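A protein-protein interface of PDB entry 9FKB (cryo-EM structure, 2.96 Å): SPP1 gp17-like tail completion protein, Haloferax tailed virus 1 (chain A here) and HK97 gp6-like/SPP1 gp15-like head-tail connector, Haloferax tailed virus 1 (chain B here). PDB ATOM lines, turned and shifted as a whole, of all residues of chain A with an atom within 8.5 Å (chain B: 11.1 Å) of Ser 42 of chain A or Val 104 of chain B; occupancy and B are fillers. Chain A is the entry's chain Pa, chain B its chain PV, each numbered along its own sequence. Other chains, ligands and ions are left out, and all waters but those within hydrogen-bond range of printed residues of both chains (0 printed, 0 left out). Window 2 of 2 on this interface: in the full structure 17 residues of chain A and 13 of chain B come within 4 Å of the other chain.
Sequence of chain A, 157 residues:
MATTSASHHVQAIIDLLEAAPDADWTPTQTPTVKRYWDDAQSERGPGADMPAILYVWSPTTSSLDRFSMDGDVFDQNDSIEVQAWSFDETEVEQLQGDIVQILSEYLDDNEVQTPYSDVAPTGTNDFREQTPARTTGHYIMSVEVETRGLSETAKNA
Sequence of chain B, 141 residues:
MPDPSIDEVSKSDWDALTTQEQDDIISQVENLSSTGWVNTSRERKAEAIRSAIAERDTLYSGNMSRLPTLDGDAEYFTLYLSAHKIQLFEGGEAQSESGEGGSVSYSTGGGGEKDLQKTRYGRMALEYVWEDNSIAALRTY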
ATOM      1  N   ASP A  39       9.219  -4.165  -6.788  1.00  0.00           N
ATOM      2  CA  ASP A  39      10.670  -4.275  -6.610  1.00  0.00           C
ATOM      3  C   ASP A  39      11.139  -3.586  -5.325  1.00  0.00           C
ATOM      4  O   ASP A  39      10.601  -2.550  -4.952  1.00  0.00           O
ATOM      5  CB  ASP A  39      11.427  -3.667  -7.799  1.00  0.00           C
ATOM      6  CG  ASP A  39      11.139  -4.290  -9.164  1.00  0.00           C
ATOM      7  OD1 ASP A  39      10.754  -5.479  -9.247  1.00  0.00           O
ATOM      8  OD2 ASP A  39      11.361  -3.587 -10.171  1.00  0.00           O
ATOM      9  N   ALA A  40      12.174  -4.141  -4.668  1.00  0.00           N
ATOM     10  CA  ALA A  40      12.770  -3.497  -3.495  1.00  0.00           C
ATOM     11  C   ALA A  40      13.786  -2.433  -3.915  1.00  0.00           C
ATOM     12  O   ALA A  40      14.370  -2.491  -4.993  1.00  0.00           O
ATOM     13  CB  ALA A  40      13.412  -4.499  -2.562  1.00  0.00           C
ATOM     14  N   GLN A  41      14.048  -1.471  -3.024  1.00  0.00           N
ATOM     15  CA  GLN A  41      14.717  -0.230  -3.403  1.00  0.00           C
ATOM     16  C   GLN A  41      16.121  -0.439  -3.996  1.00  0.00           C
ATOM     17  O   GLN A  41      16.461   0.177  -5.009  1.00  0.00           O
ATOM     18  CB  GLN A  41      14.731   0.729  -2.216  1.00  0.00           C
ATOM     19  CG  GLN A  41      15.235   2.122  -2.580  1.00  0.00           C
ATOM     20  CD  GLN A  41      14.301   2.839  -3.537  1.00  0.00           C
ATOM     21  OE1 GLN A  41      14.245   2.563  -4.742  1.00  0.00           O
ATOM     22  NE2 GLN A  41      13.547   3.794  -3.009  1.00  0.00           N
ATOM     23  N   SER A  42      16.935  -1.314  -3.386  1.00  0.00           N
ATOM     24  CA  SER A  42      18.314  -1.569  -3.811  1.00  0.00           C
ATOM     25  C   SER A  42      18.433  -2.187  -5.208  1.00  0.00           C
ATOM     26  O   SER A  42      19.537  -2.267  -5.761  1.00  0.00           O
ATOM     27  CB  SER A  42      19.057  -2.409  -2.805  1.00  0.00           C
ATOM     28  OG  SER A  42      18.925  -1.834  -1.526  1.00  0.00           O
ATOM     29  N   GLU A  43      17.306  -2.639  -5.771  1.00  0.00           N
ATOM     30  CA  GLU A  43      17.256  -3.260  -7.090  1.00  0.00           C
ATOM     31  C   GLU A  43      16.159  -2.657  -7.976  1.00  0.00           C
ATOM     32  O   GLU A  43      15.889  -3.196  -9.049  1.00  0.00           O
ATOM     33  CB  GLU A  43      17.121  -4.776  -6.932  1.00  0.00           C
ATOM     34  CG  GLU A  43      15.812  -5.230  -6.292  1.00  0.00           C
ATOM     35  CD  GLU A  43      15.762  -6.750  -6.246  1.00  0.00           C
ATOM     36  OE1 GLU A  43      15.110  -7.351  -7.127  1.00  0.00           O
ATOM     37  OE2 GLU A  43      16.399  -7.335  -5.341  1.00  0.00           O
ATOM     38  N   ARG A  44      15.558  -1.532  -7.553  1.00  0.00           N
ATOM     39  CA  ARG A  44      14.591  -0.778  -8.347  1.00  0.00           C
ATOM     40  C   ARG A  44      15.295  -0.140  -9.551  1.00  0.00           C
ATOM     41  O   ARG A  44      16.474   0.228  -9.482  1.00  0.00           O
ATOM     42  CB  ARG A  44      13.863   0.240  -7.455  1.00  0.00           C
ATOM     43  CG  ARG A  44      12.691   0.907  -8.164  1.00  0.00           C
ATOM     44  CD  ARG A  44      11.837   1.792  -7.282  1.00  0.00           C
ATOM     45  NE  ARG A  44      10.846   1.069  -6.510  1.00  0.00           N
ATOM     46  CZ  ARG A  44      10.751   1.038  -5.180  1.00  0.00           C
ATOM     47  NH1 ARG A  44       9.770   0.376  -4.599  1.00  0.00           N
ATOM     48  NH2 ARG A  44      11.608   1.667  -4.403  1.00  0.00           N
ATOM     49  N   GLY A  45      14.547   0.003 -10.658  1.00  0.00           N
ATOM     50  CA  GLY A  45      15.108   0.402 -11.939  1.00  0.00           C
ATOM     51  C   GLY A  45      15.730  -0.773 -12.688  1.00  0.00           C
ATOM     52  O   GLY A  45      16.049  -1.804 -12.102  1.00  0.00           O
ATOM     53  N   TRP A  85      12.129   4.723 -15.287  1.00  0.00           N
ATOM     54  CA  TRP A  85      13.533   4.608 -14.912  1.00  0.00           C
ATOM     55  C   TRP A  85      14.348   4.006 -16.066  1.00  0.00           C
ATOM     56  O   TRP A  85      14.014   2.938 -16.571  1.00  0.00           O
ATOM     57  CB  TRP A  85      13.684   3.714 -13.673  1.00  0.00           C
ATOM     58  CG  TRP A  85      13.116   4.170 -12.360  1.00  0.00           C
ATOM     59  CD1 TRP A  85      11.887   4.700 -12.112  1.00  0.00           C
ATOM     60  CD2 TRP A  85      13.761   4.079 -11.062  1.00  0.00           C
ATOM     61  NE1 TRP A  85      11.739   4.957 -10.770  1.00  0.00           N
ATOM     62  CE2 TRP A  85      12.858   4.553 -10.084  1.00  0.00           C
ATOM     63  CE3 TRP A  85      15.011   3.621 -10.615  1.00  0.00           C
ATOM     64  CZ2 TRP A  85      13.183   4.567  -8.713  1.00  0.00           C
ATOM     65  CZ3 TRP A  85      15.343   3.632  -9.268  1.00  0.00           C
ATOM     66  CH2 TRP A  85      14.423   4.088  -8.318  1.00  0.00           C
ATOM     67  N   HIS A 138      20.369   5.589 -12.490  1.00  0.00           N
ATOM     68  CA  HIS A 138      19.118   5.814 -13.197  1.00  0.00           C
ATOM     69  C   HIS A 138      18.769   7.296 -13.286  1.00  0.00           C
ATOM     70  O   HIS A 138      18.839   8.016 -12.304  1.00  0.00           O
ATOM     71  CB  HIS A 138      17.978   5.050 -12.526  1.00  0.00           C
ATOM     72  CG  HIS A 138      18.218   3.577 -12.488  1.00  0.00           C
ATOM     73  ND1 HIS A 138      18.560   2.882 -11.328  1.00  0.00           N
ATOM     74  CD2 HIS A 138      18.195   2.675 -13.485  1.00  0.00           C
ATOM     75  CE1 HIS A 138      18.712   1.610 -11.626  1.00  0.00           C
ATOM     76  NE2 HIS A 138      18.493   1.461 -12.944  1.00  0.00           N
ATOM     77  N   SER B  33      28.815  -5.864 -12.943  1.00  0.00           N
ATOM     78  CA  SER B  33      27.811  -5.020 -12.297  1.00  0.00           C
ATOM     79  C   SER B  33      26.484  -5.064 -13.058  1.00  0.00           C
ATOM     80  O   SER B  33      26.468  -4.991 -14.283  1.00  0.00           O
ATOM     81  CB  SER B  33      28.274  -3.600 -12.163  1.00  0.00           C
ATOM     82  OG  SER B  33      27.214  -2.826 -11.636  1.00  0.00           O
ATOM     83  N   SER B  34      25.355  -5.113 -12.334  1.00  0.00           N
ATOM     84  CA  SER B  34      24.035  -5.027 -12.955  1.00  0.00           C
ATOM     85  C   SER B  34      23.855  -3.713 -13.722  1.00  0.00           C
ATOM     86  O   SER B  34      23.117  -3.682 -14.708  1.00  0.00           O
ATOM     87  CB  SER B  34      22.936  -5.210 -11.948  1.00  0.00           C
ATOM     88  OG  SER B  34      22.913  -4.123 -11.033  1.00  0.00           O
ATOM     89  N   THR B  35      24.524  -2.646 -13.255  1.00  0.00           N
ATOM     90  CA  THR B  35      24.519  -1.329 -13.885  1.00  0.00           C
ATOM     91  C   THR B  35      25.447  -1.257 -15.105  1.00  0.00           C
ATOM     92  O   THR B  35      25.375  -0.292 -15.865  1.00  0.00           O
ATOM     93  CB  THR B  35      24.890  -0.245 -12.863  1.00  0.00           C
ATOM     94  OG1 THR B  35      26.281  -0.320 -12.546  1.00  0.00           O
ATOM     95  CG2 THR B  35      24.083  -0.320 -11.585  1.00  0.00           C
ATOM     96  N   GLU B  93      32.821   3.313  -3.886  1.00  0.00           N
ATOM     97  CA  GLU B  93      31.577   2.712  -3.424  1.00  0.00           C
ATOM     98  C   GLU B  93      30.572   3.778  -2.991  1.00  0.00           C
ATOM     99  O   GLU B  93      30.882   4.640  -2.177  1.00  0.00           O
ATOM    100  CB  GLU B  93      31.836   1.789  -2.229  1.00  0.00           C
ATOM    101  CG  GLU B  93      32.550   0.497  -2.583  1.00  0.00           C
ATOM    102  CD  GLU B  93      31.757  -0.533  -3.370  1.00  0.00           C
ATOM    103  OE1 GLU B  93      30.520  -0.388  -3.513  1.00  0.00           O
ATOM    104  OE2 GLU B  93      32.377  -1.509  -3.830  1.00  0.00           O
ATOM    105  N   ALA B  94      29.326   3.670  -3.464  1.00  0.00           N
ATOM    106  CA  ALA B  94      28.233   4.383  -2.817  1.00  0.00           C
ATOM    107  C   ALA B  94      28.009   3.816  -1.411  1.00  0.00           C
ATOM    108  O   ALA B  94      27.790   2.618  -1.260  1.00  0.00           O
ATOM    109  CB  ALA B  94      26.980   4.274  -3.661  1.00  0.00           C
ATOM    110  N   GLN B  95      28.075   4.675  -0.381  1.00  0.00           N
ATOM    111  CA  GLN B  95      27.604   4.333   0.955  1.00  0.00           C
ATOM    112  C   GLN B  95      26.090   4.545   1.034  1.00  0.00           C
ATOM    113  O   GLN B  95      25.375   3.767   1.665  1.00  0.00           O
ATOM    114  CB  GLN B  95      28.325   5.185   2.001  1.00  0.00           C
ATOM    115  CG  GLN B  95      27.768   5.022   3.420  1.00  0.00           C
ATOM    116  CD  GLN B  95      28.448   5.848   4.491  1.00  0.00           C
ATOM    117  OE1 GLN B  95      29.161   6.810   4.207  1.00  0.00           O
ATOM    118  NE2 GLN B  95      28.222   5.487   5.751  1.00  0.00           N
ATOM    119  N   SER B  96      25.613   5.641   0.413  1.00  0.00           N
ATOM    120  CA  SER B  96      24.224   6.095   0.476  1.00  0.00           C
ATOM    121  C   SER B  96      23.813   6.749  -0.849  1.00  0.00           C
ATOM    122  O   SER B  96      24.635   7.391  -1.498  1.00  0.00           O
ATOM    123  CB  SER B  96      24.047   7.029   1.646  1.00  0.00           C
ATOM    124  OG  SER B  96      22.718   7.526   1.717  1.00  0.00           O
ATOM    125  N   GLU B  97      22.538   6.576  -1.226  1.00  0.00           N
ATOM    126  CA  GLU B  97      21.924   7.206  -2.391  1.00  0.00           C
ATOM    127  C   GLU B  97      20.513   7.696  -2.050  1.00  0.00           C
ATOM    128  O   GLU B  97      19.810   7.080  -1.257  1.00  0.00           O
ATOM    129  CB  GLU B  97      21.826   6.239  -3.567  1.00  0.00           C
ATOM    130  CG  GLU B  97      23.175   5.864  -4.180  1.00  0.00           C
ATOM    131  CD  GLU B  97      23.028   4.906  -5.367  1.00  0.00           C
ATOM    132  OE1 GLU B  97      22.561   3.763  -5.155  1.00  0.00           O
ATOM    133  OE2 GLU B  97      23.364   5.301  -6.523  1.00  0.00           O
ATOM    134  N   SER B  98      20.104   8.792  -2.707  1.00  0.00           N
ATOM    135  CA  SER B  98      18.836   9.485  -2.468  1.00  0.00           C
ATOM    136  C   SER B  98      18.376  10.240  -3.731  1.00  0.00           C
ATOM    137  O   SER B  98      19.187  10.756  -4.501  1.00  0.00           O
ATOM    138  CB  SER B  98      18.974  10.394  -1.272  1.00  0.00           C
ATOM    139  OG  SER B  98      17.807  11.175  -1.064  1.00  0.00           O
ATOM    140  N   GLY B  99      17.048  10.335  -3.904  1.00  0.00           N
ATOM    141  CA  GLY B  99      16.357  10.931  -5.041  1.00  0.00           C
ATOM    142  C   GLY B  99      14.847  10.665  -4.966  1.00  0.00           C
ATOM    143  O   GLY B  99      14.368  10.039  -4.003  1.00  0.00           O
ATOM    144  N   GLU B 100      14.095  11.098  -5.996  1.00  0.00           N
ATOM    145  CA  GLU B 100      12.653  10.848  -6.077  1.00  0.00           C
ATOM    146  C   GLU B 100      12.307   9.369  -6.339  1.00  0.00           C
ATOM    147  O   GLU B 100      11.138   8.961  -6.248  1.00  0.00           O
ATOM    148  CB  GLU B 100      11.978  11.810  -7.058  1.00  0.00           C
ATOM    149  CG  GLU B 100      11.459  13.120  -6.422  1.00  0.00           C
ATOM    150  CD  GLU B 100      10.191  13.061  -5.562  1.00  0.00           C
ATOM    151  OE1 GLU B 100      10.077  12.143  -4.715  1.00  0.00           O
ATOM    152  OE2 GLU B 100       9.310  13.952  -5.720  1.00  0.00           O
ATOM    153  N   GLY B 101      13.320   8.549  -6.639  1.00  0.00           N
ATOM    154  CA  GLY B 101      13.184   7.093  -6.585  1.00  0.00           C
ATOM    155  C   GLY B 101      13.056   6.554  -5.156  1.00  0.00           C
ATOM    156  O   GLY B 101      12.542   5.456  -4.946  1.00  0.00           O
ATOM    157  N   GLY B 102      13.529   7.339  -4.182  1.00  0.00           N
ATOM    158  CA  GLY B 102      13.720   6.971  -2.786  1.00  0.00           C
ATOM    159  C   GLY B 102      15.199   6.754  -2.452  1.00  0.00           C
ATOM    160  O   GLY B 102      16.079   7.073  -3.254  1.00  0.00           O
ATOM    161  N   SER B 103      15.465   6.199  -1.252  1.00  0.00           N
ATOM    162  CA  SER B 103      16.783   6.247  -0.620  1.00  0.00           C
ATOM    163  C   SER B 103      17.246   4.886  -0.086  1.00  0.00           C
ATOM    164  O   SER B 103      16.447   4.078   0.382  1.00  0.00           O
ATOM    165  CB  SER B 103      16.815   7.296   0.459  1.00  0.00           C
ATOM    166  OG  SER B 103      16.297   8.528  -0.010  1.00  0.00           O
ATOM    167  N   VAL B 104      18.569   4.635  -0.149  1.00  0.00           N
ATOM    168  CA  VAL B 104      19.174   3.336   0.141  1.00  0.00           C
ATOM    169  C   VAL B 104      20.567   3.524   0.755  1.00  0.00           C
ATOM    170  O   VAL B 104      21.280   4.463   0.392  1.00  0.00           O
ATOM    171  CB  VAL B 104      19.207   2.437  -1.119  1.00  0.00           C
ATOM    172  CG1 VAL B 104      19.891   3.089  -2.314  1.00  0.00           C
ATOM    173  CG2 VAL B 104      19.879   1.096  -0.875  1.00  0.00           C
ATOM    174  N   SER B 105      20.979   2.583   1.631  1.00  0.00           N
ATOM    175  CA  SER B 105      22.301   2.571   2.253  1.00  0.00           C
ATOM    176  C   SER B 105      22.947   1.178   2.199  1.00  0.00           C
ATOM    177  O   SER B 105      22.291   0.188   2.507  1.00  0.00           O
ATOM    178  CB  SER B 105      22.219   3.132   3.651  1.00  0.00           C
ATOM    179  OG  SER B 105      23.496   3.138   4.272  1.00  0.00           O
ATOM    180  N   TYR B 106      24.258   1.120   1.914  1.00  0.00           N
ATOM    181  CA  TYR B 106      24.930  -0.101   1.479  1.00  0.00           C
ATOM    182  C   TYR B 106      25.847  -0.762   2.531  1.00  0.00           C
ATOM    183  O   TYR B 106      26.679  -1.599   2.159  1.00  0.00           O
ATOM    184  CB  TYR B 106      25.652   0.169   0.157  1.00  0.00           C
ATOM    185  CG  TYR B 106      24.747   0.478  -1.008  1.00  0.00           C
ATOM    186  CD1 TYR B 106      23.952  -0.509  -1.580  1.00  0.00           C
ATOM    187  CD2 TYR B 106      24.707   1.753  -1.557  1.00  0.00           C
ATOM    188  CE1 TYR B 106      23.121  -0.231  -2.662  1.00  0.00           C
ATOM    189  CE2 TYR B 106      23.913   2.036  -2.672  1.00  0.00           C
ATOM    190  CZ  TYR B 106      23.106   1.042  -3.221  1.00  0.00           C
ATOM    191  OH  TYR B 106      22.308   1.307  -4.309  1.00  0.00           O
ATOM    192  N   SER B 107      25.721  -0.395   3.827  1.00  0.00           N
ATOM    193  CA  SER B 107      26.205  -1.197   4.962  1.00  0.00           C
ATOM    194  C   SER B 107      27.734  -1.312   5.101  1.00  0.00           C
ATOM    195  O   SER B 107      28.224  -2.099   5.923  1.00  0.00           O
ATOM    196  CB  SER B 107      25.572  -2.576   4.923  1.00  0.00           C
ATOM    197  OG  SER B 107      25.772  -3.293   6.134  1.00  0.00           O
ATOM    198  N   THR B 108      28.518  -0.487   4.391  1.00  0.00           N
ATOM    199  CA  THR B 108      29.959  -0.717   4.220  1.00  0.00           C
ATOM    200  C   THR B 108      30.761  -0.658   5.529  1.00  0.00           C
ATOM    201  O   THR B 108      31.744  -1.398   5.687  1.00  0.00           O
ATOM    202  CB  THR B 108      30.582   0.221   3.177  1.00  0.00           C
ATOM    203  OG1 THR B 108      30.503   1.589   3.593  1.00  0.00           O
ATOM    204  CG2 THR B 108      29.962   0.035   1.809  1.00  0.00           C
ATOM    205  N   ARG B 120      34.109  -3.536  -3.256  1.00  0.00           N
ATOM    206  CA  ARG B 120      33.671  -4.928  -3.209  1.00  0.00           C
ATOM    207  C   ARG B 120      34.412  -5.800  -4.227  1.00  0.00           C
ATOM    208  O   ARG B 120      34.792  -6.931  -3.915  1.00  0.00           O
ATOM    209  CB  ARG B 120      32.145  -4.988  -3.349  1.00  0.00           C
ATOM    210  CG  ARG B 120      31.581  -4.553  -4.698  1.00  0.00           C
ATOM    211  CD  ARG B 120      30.178  -3.966  -4.595  1.00  0.00           C
ATOM    212  NE  ARG B 120      29.609  -3.705  -5.906  1.00  0.00           N
ATOM    213  CZ  ARG B 120      29.320  -2.526  -6.456  1.00  0.00           C
ATOM    214  NH1 ARG B 120      28.797  -2.498  -7.667  1.00  0.00           N
ATOM    215  NH2 ARG B 120      29.477  -1.387  -5.813  1.00  0.00           N
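O of Gly 101 of chain B is in hydrogen-bond range of NE2 of Gln 41 of chain A (2.7 Å).
O of Val 104 of chain B sits at hydrogen-bond distance from N of Glu 97 of chain B (2.9 Å). OG of Ser 98 of chain B is in hydrogen-bond range of OG of Ser 103 of chain B, at 3.2 Å. The backbone carbonyl oxygen (O) of Asp 39 of chain A lies within hydrogen-bond range of the guanidinium group (NH1) of Arg 44 of chain A (3.1 Å). NH2 of Arg 44 of chain A lies within hydrogen-bond range of OE1 of Gln 41 of chain A (2.8 Å).
Among the printed residues, merely in contact across the chains: Ser 42 of chain A with Val 104 of chain B (3.1 Å), Gln 41 of chain A with Gly 102 of chain B (3.2 Å), Trp 85 of chain A with Gly 101 of chain B (3.3 Å), Gln 41 of chain A with Ser 103 of chain B (3.5 Å) and Arg 44 of chain A with Gly 101 of chain B (3.9 Å).
Of chain B, only Val 104 (3.1 Å) comes within 4 Å of Ser 42 of chain A. Of chain A, only Ser 42 (3.1 Å) comes within 4 Å of Val 104 of chain B. No residue of chain B comes within 4 Å of Ala 40 of chain A. Gln 41 of chain A touches three residues of chain B. Printed residues of chain B within 4 Å of Trp 85 of chain A: Gly 101 (3.3 Å). Printed residues of chain A within 4 Å of Ser 103 of chain B: Gln 41 (3.5 Å). The nearest residue of chain A that does not touch Val 104 of chain B is Gln 41 of chain A (4.2 Å).
Hydrophobic or aromatic side chains of chain A within 4 Å of the printed part of chain B: Trp 85. Hydrophobic or aromatic side chains of chain B that line the printed part of chain A: Val 104. Among the printed residues, 6 pairs touch across the chains. Among the printed residues, no Asp or Glu carboxylate lies within 4 Å of a Lys or Arg side-chain nitrogen of the other chain.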
